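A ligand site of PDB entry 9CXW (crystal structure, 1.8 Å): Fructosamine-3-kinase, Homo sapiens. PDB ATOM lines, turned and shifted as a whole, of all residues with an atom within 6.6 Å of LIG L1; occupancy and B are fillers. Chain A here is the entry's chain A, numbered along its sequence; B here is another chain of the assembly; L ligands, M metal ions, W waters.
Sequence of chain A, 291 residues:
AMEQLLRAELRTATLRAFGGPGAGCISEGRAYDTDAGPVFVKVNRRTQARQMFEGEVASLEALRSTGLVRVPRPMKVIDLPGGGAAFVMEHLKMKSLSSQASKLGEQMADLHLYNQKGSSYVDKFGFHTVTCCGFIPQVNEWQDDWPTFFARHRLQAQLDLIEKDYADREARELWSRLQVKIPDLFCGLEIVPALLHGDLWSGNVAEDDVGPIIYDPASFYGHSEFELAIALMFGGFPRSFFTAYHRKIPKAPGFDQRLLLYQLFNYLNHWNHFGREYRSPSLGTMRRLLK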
ATOM      1  N   CYS A 133      -6.505  -1.432   4.778  1.00  0.00           N
ATOM      2  CA  CYS A 133      -7.077  -0.286   5.473  1.00  0.00           C
ATOM      3  C   CYS A 133      -6.617  -0.408   6.919  1.00  0.00           C
ATOM      4  O   CYS A 133      -6.925  -1.401   7.605  1.00  0.00           O
ATOM      5  CB  CYS A 133      -8.600  -0.180   5.358  1.00  0.00           C
ATOM      6  SG  CYS A 133      -9.098   1.599   5.468  1.00  0.00           S
ATOM      7  N   GLY A 134      -5.765   0.538   7.331  1.00  0.00           N
ATOM      8  CA  GLY A 134      -5.062   0.403   8.598  1.00  0.00           C
ATOM      9  C   GLY A 134      -4.283  -0.899   8.645  1.00  0.00           C
ATOM     10  O   GLY A 134      -3.399  -1.158   7.823  1.00  0.00           O
ATOM     11  N   PHE A 135      -4.634  -1.763   9.594  1.00  0.00           N
ATOM     12  CA  PHE A 135      -3.934  -3.036   9.798  1.00  0.00           C
ATOM     13  C   PHE A 135      -4.661  -4.252   9.246  1.00  0.00           C
ATOM     14  O   PHE A 135      -4.197  -5.372   9.482  1.00  0.00           O
ATOM     15  CB  PHE A 135      -3.679  -3.237  11.306  1.00  0.00           C
ATOM     16  CG  PHE A 135      -2.533  -4.144  11.603  1.00  0.00           C
ATOM     17  CD1 PHE A 135      -1.221  -3.727  11.427  1.00  0.00           C
ATOM     18  CD2 PHE A 135      -2.772  -5.445  12.056  1.00  0.00           C
ATOM     19  CE1 PHE A 135      -0.150  -4.586  11.695  1.00  0.00           C
ATOM     20  CE2 PHE A 135      -1.705  -6.309  12.331  1.00  0.00           C
ATOM     21  CZ  PHE A 135      -0.395  -5.880  12.151  1.00  0.00           C
ATOM     22  N   GLY A 198      -8.108   6.053  -0.697  1.00  0.00           N
ATOM     23  CA  GLY A 198      -8.653   4.933   0.078  1.00  0.00           C
ATOM     24  C   GLY A 198      -8.714   5.131   1.591  1.00  0.00           C
ATOM     25  O   GLY A 198      -9.401   4.367   2.284  1.00  0.00           O
ATOM     26  N   ASP A 199      -8.061   6.154   2.119  1.00  0.00           N
ATOM     27  CA  ASP A 199      -8.059   6.370   3.553  1.00  0.00           C
ATOM     28  C   ASP A 199      -7.866   7.858   3.846  1.00  0.00           C
ATOM     29  O   ASP A 199      -6.999   8.250   4.644  1.00  0.00           O
ATOM     30  CB  ASP A 199      -6.950   5.546   4.220  1.00  0.00           C
ATOM     31  CG  ASP A 199      -7.157   5.383   5.752  1.00  0.00           C
ATOM     32  OD1 ASP A 199      -8.310   5.549   6.213  1.00  0.00           O
ATOM     33  OD2 ASP A 199      -6.176   5.089   6.454  1.00  0.00           O
ATOM     34  N   TRP A 201      -8.598  10.340   5.631  1.00  0.00           N
ATOM     35  CA  TRP A 201      -9.009  11.185   6.756  1.00  0.00           C
ATOM     36  C   TRP A 201      -8.005  12.338   7.001  1.00  0.00           C
ATOM     37  O   TRP A 201      -6.924  12.426   6.392  1.00  0.00           O
ATOM     38  CB  TRP A 201      -9.245  10.344   8.021  1.00  0.00           C
ATOM     39  CG  TRP A 201      -8.025   9.966   8.752  1.00  0.00           C
ATOM     40  CD1 TRP A 201      -7.043   9.106   8.321  1.00  0.00           C
ATOM     41  CD2 TRP A 201      -7.619  10.394  10.077  1.00  0.00           C
ATOM     42  NE1 TRP A 201      -6.052   8.988   9.300  1.00  0.00           N
ATOM     43  CE2 TRP A 201      -6.368   9.777  10.355  1.00  0.00           C
ATOM     44  CE3 TRP A 201      -8.171  11.259  11.040  1.00  0.00           C
ATOM     45  CZ2 TRP A 201      -5.667   9.974  11.596  1.00  0.00           C
ATOM     46  CZ3 TRP A 201      -7.470  11.455  12.251  1.00  0.00           C
ATOM     47  CH2 TRP A 201      -6.241  10.806  12.504  1.00  0.00           C
ATOM     48  N   ASN A 204      -4.290  11.974   7.366  1.00  0.00           N
ATOM     49  CA  ASN A 204      -3.488  11.446   6.261  1.00  0.00           C
ATOM     50  C   ASN A 204      -3.282  12.472   5.157  1.00  0.00           C
ATOM     51  O   ASN A 204      -2.904  12.114   4.025  1.00  0.00           O
ATOM     52  CB  ASN A 204      -4.133  10.194   5.693  1.00  0.00           C
ATOM     53  CG  ASN A 204      -3.907   8.971   6.574  1.00  0.00           C
ATOM     54  OD1 ASN A 204      -3.044   8.987   7.456  1.00  0.00           O
ATOM     55  ND2 ASN A 204      -4.691   7.941   6.372  1.00  0.00           N
ATOM     56  N   ASP A 216      -0.069   7.671   3.364  1.00  0.00           N
ATOM     57  CA  ASP A 216      -0.670   6.511   4.015  1.00  0.00           C
ATOM     58  C   ASP A 216      -1.889   6.006   3.255  1.00  0.00           C
ATOM     59  O   ASP A 216      -2.953   5.771   3.860  1.00  0.00           O
ATOM     60  CB  ASP A 216      -1.054   6.873   5.450  1.00  0.00           C
ATOM     61  CG  ASP A 216      -1.256   5.625   6.374  1.00  0.00           C
ATOM     62  OD1 ASP A 216      -0.778   4.507   6.043  1.00  0.00           O
ATOM     63  OD2 ASP A 216      -1.847   5.806   7.477  1.00  0.00           O
ATOM     64  N   ILE A 230     -14.850   9.129   4.869  1.00  0.00           N
ATOM     65  CA  ILE A 230     -14.003   9.231   6.063  1.00  0.00           C
ATOM     66  C   ILE A 230     -13.566  10.678   6.298  1.00  0.00           C
ATOM     67  O   ILE A 230     -13.432  11.121   7.456  1.00  0.00           O
ATOM     68  CB  ILE A 230     -12.825   8.234   5.967  1.00  0.00           C
ATOM     69  CG1 ILE A 230     -12.120   8.105   7.341  1.00  0.00           C
ATOM     70  CG2 ILE A 230     -11.802   8.651   4.894  1.00  0.00           C
ATOM     71  CD1 ILE A 230     -11.114   6.928   7.407  1.00  0.00           C
ATOM     72  N   PHE A 234     -14.904  12.156  10.169  1.00  0.00           N
ATOM     73  CA  PHE A 234     -14.025  12.488  11.294  1.00  0.00           C
ATOM     74  C   PHE A 234     -13.592  13.952  11.339  1.00  0.00           C
ATOM     75  O   PHE A 234     -12.805  14.326  12.220  1.00  0.00           O
ATOM     76  CB  PHE A 234     -12.807  11.563  11.312  1.00  0.00           C
ATOM     77  CG  PHE A 234     -13.174  10.115  11.578  1.00  0.00           C
ATOM     78  CD1 PHE A 234     -13.863   9.762  12.748  1.00  0.00           C
ATOM     79  CD2 PHE A 234     -12.845   9.103  10.679  1.00  0.00           C
ATOM     80  CE1 PHE A 234     -14.204   8.441  13.011  1.00  0.00           C
ATOM     81  CE2 PHE A 234     -13.184   7.793  10.952  1.00  0.00           C
ATOM     82  CZ  PHE A 234     -13.861   7.458  12.131  1.00  0.00           C
ATOM     83  N   ASN A 266     -16.531   2.489   7.335  1.00  0.00           N
ATOM     84  CA  ASN A 266     -15.468   3.014   8.200  1.00  0.00           C
ATOM     85  C   ASN A 266     -15.757   2.769   9.687  1.00  0.00           C
ATOM     86  O   ASN A 266     -14.833   2.450  10.465  1.00  0.00           O
ATOM     87  CB  ASN A 266     -15.246   4.496   7.912  1.00  0.00           C
ATOM     88  CG  ASN A 266     -14.522   4.704   6.590  1.00  0.00           C
ATOM     89  OD1 ASN A 266     -13.332   4.401   6.491  1.00  0.00           O
ATOM     90  ND2 ASN A 266     -15.253   5.196   5.551  1.00  0.00           N
ATOM     91  N   ASN A 269     -14.830  -0.831  10.286  1.00  0.00           N
ATOM     92  CA  ASN A 269     -13.376  -0.957  10.331  1.00  0.00           C
ATOM     93  C   ASN A 269     -12.831  -0.464  11.660  1.00  0.00           C
ATOM     94  O   ASN A 269     -11.877  -1.031  12.208  1.00  0.00           O
ATOM     95  CB  ASN A 269     -12.758  -0.149   9.162  1.00  0.00           C
ATOM     96  CG  ASN A 269     -11.265  -0.395   8.978  1.00  0.00           C
ATOM     97  OD1 ASN A 269     -10.810  -1.529   8.994  1.00  0.00           O
ATOM     98  ND2 ASN A 269     -10.497   0.685   8.753  1.00  0.00           N
ATOM     99  N   HIS A 270     -13.417   0.577  12.210  1.00  0.00           N
ATOM    100  CA  HIS A 270     -12.953   1.078  13.502  1.00  0.00           C
ATOM    101  C   HIS A 270     -13.354   0.153  14.644  1.00  0.00           C
ATOM    102  O   HIS A 270     -12.614   0.021  15.616  1.00  0.00           O
ATOM    103  CB  HIS A 270     -13.481   2.491  13.720  1.00  0.00           C
ATOM    104  CG  HIS A 270     -12.621   3.531  13.092  1.00  0.00           C
ATOM    105  ND1 HIS A 270     -12.449   3.635  11.719  1.00  0.00           N
ATOM    106  CD2 HIS A 270     -11.774   4.448  13.648  1.00  0.00           C
ATOM    107  CE1 HIS A 270     -11.572   4.597  11.466  1.00  0.00           C
ATOM    108  NE2 HIS A 270     -11.149   5.107  12.612  1.00  0.00           N
ATOM    109  N   HIS A 273     -10.808  -2.546  14.467  1.00  0.00           N
ATOM    110  CA  HIS A 273      -9.484  -2.080  14.933  1.00  0.00           C
ATOM    111  C   HIS A 273      -9.430  -1.731  16.426  1.00  0.00           C
ATOM    112  O   HIS A 273      -8.433  -2.024  17.094  1.00  0.00           O
ATOM    113  CB  HIS A 273      -9.035  -0.861  14.134  1.00  0.00           C
ATOM    114  CG  HIS A 273      -8.375  -1.223  12.837  1.00  0.00           C
ATOM    115  ND1 HIS A 273      -9.080  -1.501  11.681  1.00  0.00           N
ATOM    116  CD2 HIS A 273      -7.055  -1.318  12.503  1.00  0.00           C
ATOM    117  CE1 HIS A 273      -8.235  -1.756  10.697  1.00  0.00           C
ATOM    118  NE2 HIS A 273      -7.003  -1.675  11.176  1.00  0.00           N
ATOM    119  N   PHE A 274     -10.419  -1.017  16.927  1.00  0.00           N
ATOM    120  CA  PHE A 274     -10.388  -0.367  18.225  1.00  0.00           C
ATOM    121  C   PHE A 274     -11.435  -0.884  19.211  1.00  0.00           C
ATOM    122  O   PHE A 274     -11.420  -0.450  20.367  1.00  0.00           O
ATOM    123  CB  PHE A 274     -10.561   1.143  18.062  1.00  0.00           C
ATOM    124  CG  PHE A 274      -9.587   1.743  17.094  1.00  0.00           C
ATOM    125  CD1 PHE A 274      -8.220   1.767  17.396  1.00  0.00           C
ATOM    126  CD2 PHE A 274     -10.008   2.194  15.844  1.00  0.00           C
ATOM    127  CE1 PHE A 274      -7.300   2.267  16.498  1.00  0.00           C
ATOM    128  CE2 PHE A 274      -9.089   2.708  14.943  1.00  0.00           C
ATOM    129  CZ  PHE A 274      -7.738   2.741  15.259  1.00  0.00           C
ATOM    130  N   TYR A 278     -16.901   1.577  18.918  1.00  0.00           N
ATOM    131  CA  TYR A 278     -17.503   1.853  17.602  1.00  0.00           C
ATOM    132  C   TYR A 278     -18.690   0.962  17.298  1.00  0.00           C
ATOM    133  O   TYR A 278     -19.199   0.973  16.159  1.00  0.00           O
ATOM    134  CB  TYR A 278     -16.452   1.719  16.520  1.00  0.00           C
ATOM    135  CG  TYR A 278     -15.458   2.830  16.607  1.00  0.00           C
ATOM    136  CD1 TYR A 278     -15.723   4.063  16.018  1.00  0.00           C
ATOM    137  CD2 TYR A 278     -14.267   2.683  17.339  1.00  0.00           C
ATOM    138  CE1 TYR A 278     -14.831   5.099  16.126  1.00  0.00           C
ATOM    139  CE2 TYR A 278     -13.363   3.714  17.420  1.00  0.00           C
ATOM    140  CZ  TYR A 278     -13.642   4.918  16.812  1.00  0.00           C
ATOM    141  OH  TYR A 278     -12.752   5.953  16.891  1.00  0.00           O
ATOM    142  N   PHE B 274      -4.055   1.912  20.654  1.00  0.00           N
ATOM    143  CA  PHE B 274      -3.832   1.924  19.214  1.00  0.00           C
ATOM    144  C   PHE B 274      -4.456   0.759  18.461  1.00  0.00           C
ATOM    145  O   PHE B 274      -4.340   0.715  17.229  1.00  0.00           O
ATOM    146  CB  PHE B 274      -2.316   1.938  18.910  1.00  0.00           C
ATOM    147  CG  PHE B 274      -1.596   3.099  19.540  1.00  0.00           C
ATOM    148  CD1 PHE B 274      -1.975   4.407  19.270  1.00  0.00           C
ATOM    149  CD2 PHE B 274      -0.544   2.898  20.421  1.00  0.00           C
ATOM    150  CE1 PHE B 274      -1.341   5.504  19.868  1.00  0.00           C
ATOM    151  CE2 PHE B 274       0.097   3.988  21.045  1.00  0.00           C
ATOM    152  CZ  PHE B 274      -0.297   5.291  20.763  1.00  0.00           C
HETATM  153  N1  LIG L   1      -8.954   6.851  12.826  1.00  0.00           N
HETATM  154  C1  LIG L   1      -8.479   6.717  11.396  1.00  0.00           C
HETATM  155  C2  LIG L   1      -7.309   5.726  11.039  1.00  0.00           C
HETATM  156  O1  LIG L   1      -6.455   5.325  11.852  1.00  0.00           O
HETATM  157  C3  LIG L   1      -7.897   7.062  13.813  1.00  0.00           C
HETATM  158  C4  LIG L   1      -8.455   7.256  15.235  1.00  0.00           C
HETATM  159  C5  LIG L   1     -10.119   8.657  14.222  1.00  0.00           C
HETATM  160  C6  LIG L   1      -9.840   8.043  12.838  1.00  0.00           C
HETATM  161  C7  LIG L   1      -7.202   5.321   9.528  1.00  0.00           C
HETATM  162  C8  LIG L   1      -8.010   4.043   9.094  1.00  0.00           C
HETATM  163  C9  LIG L   1      -8.294   2.956  10.201  1.00  0.00           C
HETATM  164  C10 LIG L   1      -7.051   2.151  10.613  1.00  0.00           C
HETATM  165  O2  LIG L   1      -9.833   7.700  15.239  1.00  0.00           O
HETATM  166  O3  LIG L   1      -6.100   2.936  11.341  1.00  0.00           O
HETATM  167  O4  LIG L   1      -8.901   3.526  11.365  1.00  0.00           O
HETATM  168  O5  LIG L   1      -9.243   4.479   8.478  1.00  0.00           O
HETATM  169  O6  LIG L   1      -5.817   5.182   9.075  1.00  0.00           O
HETATM  170  P1  LG2 L   2       0.636   5.850  10.510  1.00  0.00           P
HETATM  171  O1  LG2 L   2      -0.667   6.598  10.679  1.00  0.00           O
HETATM  172  O2  LG2 L   2       0.560   4.611   9.634  1.00  0.00           O
HETATM  173  O3  LG2 L   2       1.305   5.570  11.831  1.00  0.00           O
HETATM  174  P2  LG2 L   2       1.311   7.988   8.582  1.00  0.00           P
HETATM  175  O4  LG2 L   2       1.935   7.580   7.268  1.00  0.00           O
HETATM  176  O5  LG2 L   2      -0.147   8.374   8.606  1.00  0.00           O
HETATM  177  O6  LG2 L   2       1.662   6.864   9.719  1.00  0.00           O
HETATM  178  O7  LG2 L   2       2.155   9.270   9.098  1.00  0.00           O
HETATM  179  C1  LG2 L   2       1.823   9.887  10.354  1.00  0.00           C
HETATM  180  C2  LG2 L   2       2.619  11.174  10.544  1.00  0.00           C
HETATM  181  O8  LG2 L   2       3.980  10.927  10.228  1.00  0.00           O
HETATM  182  C3  LG2 L   2       2.208  12.296   9.602  1.00  0.00           C
HETATM  183  O9  LG2 L   2       1.111  13.067  10.094  1.00  0.00           O
HETATM  184  C4  LG2 L   2       3.485  13.099   9.400  1.00  0.00           C
HETATM  185  O10 LG2 L   2       3.715  14.170  10.343  1.00  0.00           O
HETATM  186  C5  LG2 L   2       4.561  12.043   9.556  1.00  0.00           C
HETATM  187  N1  LG2 L   2       4.995  11.599   8.206  1.00  0.00           N
HETATM  188  C6  LG2 L   2       4.472  10.561   7.520  1.00  0.00           C
HETATM  189  N2  LG2 L   2       5.104  10.380   6.339  1.00  0.00           N
HETATM  190  C7  LG2 L   2       6.024  11.345   6.240  1.00  0.00           C
HETATM  191  C8  LG2 L   2       7.028  11.732   5.232  1.00  0.00           C
HETATM  192  N3  LG2 L   2       7.127  10.997   4.104  1.00  0.00           N
HETATM  193  N4  LG2 L   2       7.842  12.797   5.496  1.00  0.00           N
HETATM  194  C9  LG2 L   2       7.706  13.466   6.647  1.00  0.00           C
HETATM  195  N5  LG2 L   2       6.794  13.164   7.594  1.00  0.00           N
HETATM  196  C10 LG2 L   2       5.965  12.127   7.476  1.00  0.00           C
HETATM  197 MG    MG M   1      -1.944   7.565   8.948  1.00  0.00          MG
HETATM  198  O   HOH W   1      -3.952   6.818   9.443  1.00  0.00           O
HETATM  199  O   HOH W   2     -11.906   3.356   8.525  1.00  0.00           O
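O of Asp 199 is in hydrogen-bond range of ND2 of Asn 204 (2.9 Å).
A ring nitrogen (ND1) of His 270 lies within hydrogen-bond range of the backbone carbonyl oxygen of Asn 266, 2.9 Å away.
O of Asn 269 lies within hydrogen-bond range of ND1 of His 273.
The side-chain sulfur (SG) of Cys 133 is in hydrogen-bond range of the side-chain amide nitrogen (ND2) of Asn 269, at 3.7 Å.
The side-chain amide nitrogen (ND2) of Asn 204 sits close to the indole nitrogen (NE1) of Trp 201, 3.4 Å away.
NE2 of His 273 sits at hydrogen-bond distance from N of Phe 135 (2.9 Å).
An oxygen (O6) of LIG L1 lies within hydrogen-bond range of the side-chain carboxylate of Asp 199, at 2.6 Å.
O4 of LIG L1 sits close to NE2 of His 270 (3.0 Å).
Water W1 lies within hydrogen-bond range of an oxygen (O6) of LIG L1 (2.5 Å), the indole nitrogen of Trp 201 (3.0 Å) and the side-chain amide nitrogen of Asn 204 (3.4 Å).
Water W2 lies within hydrogen-bond range of OD1 of Asn 266, O5 of LIG L1, ND2 of Asn 269 and ND1 of His 270.
Gly 134 touches LIG L1 (CA to C10, 3.3 Å).
Trp 201 touches LIG L1.
Ile 230 touches LIG L1.
Phe 234 touches LIG L1 (CE2 to C6, 3.8 Å).
Asn 269 touches LIG L1.
NE2 of His 273 touches C10 of LIG L1 (3.9 Å).
Phe 274 of chain A touches LIG L1 (CE2 to O4, 3.7 Å).
Tyr 278 touches LIG L1 (OH to O2, 3.8 Å).
Hydrophobic or aromatic side chains within 4 Å of LIG L1: Trp 201, Ile 230, Phe 234, His 270, His 273 and Phe 274 of chain A.
Ten residues have an atom within 4 Å of LIG L1: Gly 134, Asp 199, Trp 201, Ile 230, Phe 234, Asn 269, His 270, His 273, Phe 274 of chain A and Tyr 278.
The nearest printed residue that does not touch LIG L1 is Asn 204 (4.02 Å).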
